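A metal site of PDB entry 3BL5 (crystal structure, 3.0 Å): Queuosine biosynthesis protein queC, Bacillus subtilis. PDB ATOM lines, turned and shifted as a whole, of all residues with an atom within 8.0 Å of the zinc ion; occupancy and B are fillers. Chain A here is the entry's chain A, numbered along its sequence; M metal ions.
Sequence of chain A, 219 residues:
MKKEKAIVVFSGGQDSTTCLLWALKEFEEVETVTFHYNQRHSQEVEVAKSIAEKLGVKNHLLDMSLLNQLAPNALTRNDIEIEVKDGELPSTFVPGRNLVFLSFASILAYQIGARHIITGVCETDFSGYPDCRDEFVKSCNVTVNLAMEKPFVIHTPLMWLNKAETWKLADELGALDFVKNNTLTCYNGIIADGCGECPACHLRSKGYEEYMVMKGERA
Merely in contact with the zinc ion: Tyr 187 (3.4 Å) and Asn 188 (3.4 Å). Six residues have an atom within 4 Å of the zinc ion: Cys 186, Tyr 187, Asn 188, Cys 195, Cys 198 and Cys 201. The nearest printed residue that does not touch the zinc ion is Gly 196 (4.1 Å).
SG of Cys 198 is bound to the zinc ion (2.3 Å). The zinc ion is bound by SG of Cys 201 (2.3 Å). SG of Cys 195 binds the zinc ion (2.4 Å). SG of Cys 186 is bound to the zinc ion, at 2.4 Å. The zinc ion has four donor atoms within binding distance.
The side-chain sulfur of Cys 198 lies close to the backbone NH of Tyr 187 (3.5 Å). The side-chain sulfur (SG) of Cys 201 sits close to the backbone NH (N) of Gly 196. The backbone NH (N) of Glu 197 lies close to the side-chain sulfur (SG) of Cys 195 (2.9 Å). The side-chain sulfur of Cys 186 sits close to the backbone NH of Asn 188.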
ATOM      1  N   LEU A 184     -18.277   7.756   4.385  1.00  0.00           N
ATOM      2  CA  LEU A 184     -19.628   7.543   3.909  1.00  0.00           C
ATOM      3  C   LEU A 184     -20.095   6.148   4.328  1.00  0.00           C
ATOM      4  O   LEU A 184     -19.541   5.138   3.885  1.00  0.00           O
ATOM      5  CB  LEU A 184     -19.666   7.675   2.389  1.00  0.00           C
ATOM      6  CG  LEU A 184     -20.941   7.302   1.642  1.00  0.00           C
ATOM      7  CD1 LEU A 184     -22.176   7.823   2.363  1.00  0.00           C
ATOM      8  CD2 LEU A 184     -20.843   7.853   0.230  1.00  0.00           C
ATOM      9  N   THR A 185     -21.107   6.094   5.195  1.00  0.00           N
ATOM     10  CA  THR A 185     -21.648   4.832   5.686  1.00  0.00           C
ATOM     11  C   THR A 185     -23.097   4.667   5.256  1.00  0.00           C
ATOM     12  O   THR A 185     -23.496   3.587   4.840  1.00  0.00           O
ATOM     13  CB  THR A 185     -21.557   4.774   7.214  1.00  0.00           C
ATOM     14  OG1 THR A 185     -20.182   4.729   7.610  1.00  0.00           O
ATOM     15  CG2 THR A 185     -22.267   3.550   7.739  1.00  0.00           C
ATOM     16  N   CYS A 186     -23.866   5.740   5.379  1.00  0.00           N
ATOM     17  CA  CYS A 186     -25.290   5.749   5.018  1.00  0.00           C
ATOM     18  C   CYS A 186     -25.545   5.087   3.677  1.00  0.00           C
ATOM     19  O   CYS A 186     -24.672   5.092   2.792  1.00  0.00           O
ATOM     20  CB  CYS A 186     -25.807   7.187   4.968  1.00  0.00           C
ATOM     21  SG  CYS A 186     -27.458   7.394   4.219  1.00  0.00           S
ATOM     22  N   TYR A 187     -26.732   4.519   3.515  1.00  0.00           N
ATOM     23  CA  TYR A 187     -27.098   3.855   2.272  1.00  0.00           C
ATOM     24  C   TYR A 187     -27.724   4.844   1.285  1.00  0.00           C
ATOM     25  O   TYR A 187     -28.383   4.446   0.320  1.00  0.00           O
ATOM     26  CB  TYR A 187     -28.069   2.692   2.526  1.00  0.00           C
ATOM     27  CG  TYR A 187     -27.433   1.415   3.050  1.00  0.00           C
ATOM     28  CD1 TYR A 187     -26.314   0.860   2.413  1.00  0.00           C
ATOM     29  CD2 TYR A 187     -27.975   0.735   4.149  1.00  0.00           C
ATOM     30  CE1 TYR A 187     -25.750  -0.345   2.857  1.00  0.00           C
ATOM     31  CE2 TYR A 187     -27.412  -0.468   4.604  1.00  0.00           C
ATOM     32  CZ  TYR A 187     -26.306  -0.993   3.949  1.00  0.00           C
ATOM     33  OH  TYR A 187     -25.747  -2.166   4.397  1.00  0.00           O
ATOM     34  N   ASN A 188     -27.517   6.134   1.517  1.00  0.00           N
ATOM     35  CA  ASN A 188     -28.097   7.146   0.641  1.00  0.00           C
ATOM     36  C   ASN A 188     -27.154   8.308   0.354  1.00  0.00           C
ATOM     37  O   ASN A 188     -27.567   9.471   0.436  1.00  0.00           O
ATOM     38  CB  ASN A 188     -29.382   7.677   1.254  1.00  0.00           C
ATOM     39  CG  ASN A 188     -30.264   6.581   1.786  1.00  0.00           C
ATOM     40  OD1 ASN A 188     -29.899   5.884   2.741  1.00  0.00           O
ATOM     41  ND2 ASN A 188     -31.435   6.399   1.170  1.00  0.00           N
ATOM     42  N   GLY A 189     -25.903   8.015   0.028  1.00  0.00           N
ATOM     43  CA  GLY A 189     -24.947   9.065  -0.287  1.00  0.00           C
ATOM     44  C   GLY A 189     -24.786  10.147   0.771  1.00  0.00           C
ATOM     45  O   GLY A 189     -24.004  11.080   0.583  1.00  0.00           O
ATOM     46  N   ILE A 190     -25.524  10.033   1.869  1.00  0.00           N
ATOM     47  CA  ILE A 190     -25.458  11.006   2.964  1.00  0.00           C
ATOM     48  C   ILE A 190     -24.239  10.722   3.850  1.00  0.00           C
ATOM     49  O   ILE A 190     -24.213   9.741   4.599  1.00  0.00           O
ATOM     50  CB  ILE A 190     -26.725  10.965   3.856  1.00  0.00           C
ATOM     51  CG1 ILE A 190     -27.982  11.158   2.997  1.00  0.00           C
ATOM     52  CG2 ILE A 190     -26.672  12.065   4.895  1.00  0.00           C
ATOM     53  CD1 ILE A 190     -29.265  10.896   3.749  1.00  0.00           C
ATOM     54  N   ILE A 191     -23.241  11.599   3.756  1.00  0.00           N
ATOM     55  CA  ILE A 191     -22.014  11.477   4.518  1.00  0.00           C
ATOM     56  C   ILE A 191     -22.236  11.538   6.026  1.00  0.00           C
ATOM     57  O   ILE A 191     -23.232  12.079   6.499  1.00  0.00           O
ATOM     58  CB  ILE A 191     -21.020  12.576   4.114  1.00  0.00           C
ATOM     59  CG1 ILE A 191     -20.758  12.506   2.599  1.00  0.00           C
ATOM     60  CG2 ILE A 191     -19.709  12.402   4.859  1.00  0.00           C
ATOM     61  CD1 ILE A 191     -20.154  11.190   2.128  1.00  0.00           C
ATOM     62  N   ALA A 192     -21.303  10.963   6.782  1.00  0.00           N
ATOM     63  CA  ALA A 192     -21.382  10.944   8.232  1.00  0.00           C
ATOM     64  C   ALA A 192     -22.692  10.332   8.695  1.00  0.00           C
ATOM     65  O   ALA A 192     -23.053   9.235   8.284  1.00  0.00           O
ATOM     66  CB  ALA A 192     -21.242  12.345   8.765  1.00  0.00           C
ATOM     67  N   ASP A 193     -23.403  11.060   9.564  1.00  0.00           N
ATOM     68  CA  ASP A 193     -24.683  10.601  10.101  1.00  0.00           C
ATOM     69  C   ASP A 193     -25.715  10.670   8.982  1.00  0.00           C
ATOM     70  O   ASP A 193     -26.504  11.599   8.928  1.00  0.00           O
ATOM     71  CB  ASP A 193     -25.157  11.529  11.228  1.00  0.00           C
ATOM     72  CG  ASP A 193     -24.070  11.832  12.234  1.00  0.00           C
ATOM     73  OD1 ASP A 193     -24.318  12.664  13.137  1.00  0.00           O
ATOM     74  OD2 ASP A 193     -22.973  11.237  12.125  1.00  0.00           O
ATOM     75  N   GLY A 194     -25.688   9.686   8.088  1.00  0.00           N
ATOM     76  CA  GLY A 194     -26.629   9.697   6.975  1.00  0.00           C
ATOM     77  C   GLY A 194     -28.104   9.882   7.321  1.00  0.00           C
ATOM     78  O   GLY A 194     -28.461  10.577   8.267  1.00  0.00           O
ATOM     79  N   CYS A 195     -28.954   9.244   6.538  1.00  0.00           N
ATOM     80  CA  CYS A 195     -30.396   9.311   6.736  1.00  0.00           C
ATOM     81  C   CYS A 195     -30.805   9.163   8.205  1.00  0.00           C
ATOM     82  O   CYS A 195     -31.681   9.872   8.701  1.00  0.00           O
ATOM     83  CB  CYS A 195     -31.097   8.222   5.907  1.00  0.00           C
ATOM     84  SG  CYS A 195     -30.762   6.520   6.450  1.00  0.00           S
ATOM     85  N   GLY A 196     -30.141   8.246   8.903  1.00  0.00           N
ATOM     86  CA  GLY A 196     -30.486   8.017  10.289  1.00  0.00           C
ATOM     87  C   GLY A 196     -31.679   7.085  10.282  1.00  0.00           C
ATOM     88  O   GLY A 196     -32.428   7.010  11.249  1.00  0.00           O
ATOM     89  N   GLU A 197     -31.837   6.384   9.158  1.00  0.00           N
ATOM     90  CA  GLU A 197     -32.932   5.445   8.943  1.00  0.00           C
ATOM     91  C   GLU A 197     -32.431   4.037   8.639  1.00  0.00           C
ATOM     92  O   GLU A 197     -32.641   3.105   9.407  1.00  0.00           O
ATOM     93  CB  GLU A 197     -33.808   5.910   7.773  1.00  0.00           C
ATOM     94  CG  GLU A 197     -35.212   6.350   8.174  1.00  0.00           C
ATOM     95  CD  GLU A 197     -35.218   7.663   8.911  1.00  0.00           C
ATOM     96  OE1 GLU A 197     -34.737   8.663   8.337  1.00  0.00           O
ATOM     97  OE2 GLU A 197     -35.708   7.708  10.061  1.00  0.00           O
ATOM     98  N   CYS A 198     -31.765   3.897   7.496  1.00  0.00           N
ATOM     99  CA  CYS A 198     -31.236   2.617   7.024  1.00  0.00           C
ATOM    100  C   CYS A 198     -30.503   1.809   8.092  1.00  0.00           C
ATOM    101  O   CYS A 198     -30.226   2.307   9.191  1.00  0.00           O
ATOM    102  CB  CYS A 198     -30.295   2.862   5.839  1.00  0.00           C
ATOM    103  SG  CYS A 198     -28.832   3.836   6.230  1.00  0.00           S
ATOM    104  N   PRO A 199     -30.191   0.541   7.791  1.00  0.00           N
ATOM    105  CA  PRO A 199     -29.486  -0.303   8.752  1.00  0.00           C
ATOM    106  C   PRO A 199     -28.130   0.312   9.057  1.00  0.00           C
ATOM    107  O   PRO A 199     -27.828   0.630  10.213  1.00  0.00           O
ATOM    108  CB  PRO A 199     -29.351  -1.628   8.025  1.00  0.00           C
ATOM    109  CG  PRO A 199     -30.502  -1.628   7.077  1.00  0.00           C
ATOM    110  CD  PRO A 199     -30.483  -0.217   6.560  1.00  0.00           C
ATOM    111  N   ALA A 200     -27.326   0.486   8.011  1.00  0.00           N
ATOM    112  CA  ALA A 200     -25.999   1.070   8.126  1.00  0.00           C
ATOM    113  C   ALA A 200     -25.960   2.168   9.195  1.00  0.00           C
ATOM    114  O   ALA A 200     -25.218   2.068  10.182  1.00  0.00           O
ATOM    115  CB  ALA A 200     -25.569   1.630   6.770  1.00  0.00           C
ATOM    116  N   CYS A 201     -26.756   3.216   8.994  1.00  0.00           N
ATOM    117  CA  CYS A 201     -26.823   4.340   9.929  1.00  0.00           C
ATOM    118  C   CYS A 201     -27.063   3.913  11.361  1.00  0.00           C
ATOM    119  O   CYS A 201     -26.339   4.309  12.269  1.00  0.00           O
ATOM    120  CB  CYS A 201     -27.918   5.321   9.513  1.00  0.00           C
ATOM    121  SG  CYS A 201     -27.571   6.252   8.006  1.00  0.00           S
ATOM    122  N   HIS A 202     -28.091   3.105  11.572  1.00  0.00           N
ATOM    123  CA  HIS A 202     -28.423   2.624  12.897  1.00  0.00           C
ATOM    124  C   HIS A 202     -27.253   1.886  13.525  1.00  0.00           C
ATOM    125  O   HIS A 202     -26.905   2.124  14.690  1.00  0.00           O
ATOM    126  CB  HIS A 202     -29.649   1.707  12.824  1.00  0.00           C
ATOM    127  CG  HIS A 202     -30.941   2.440  12.641  1.00  0.00           C
ATOM    128  ND1 HIS A 202     -32.140   1.784  12.445  1.00  0.00           N
ATOM    129  CD2 HIS A 202     -31.229   3.763  12.657  1.00  0.00           C
ATOM    130  CE1 HIS A 202     -33.115   2.678  12.338  1.00  0.00           C
ATOM    131  NE2 HIS A 202     -32.586   3.884  12.460  1.00  0.00           N
HETATM  132 ZN    ZN M   1     -28.508   6.081   5.888  1.00  0.00          ZN
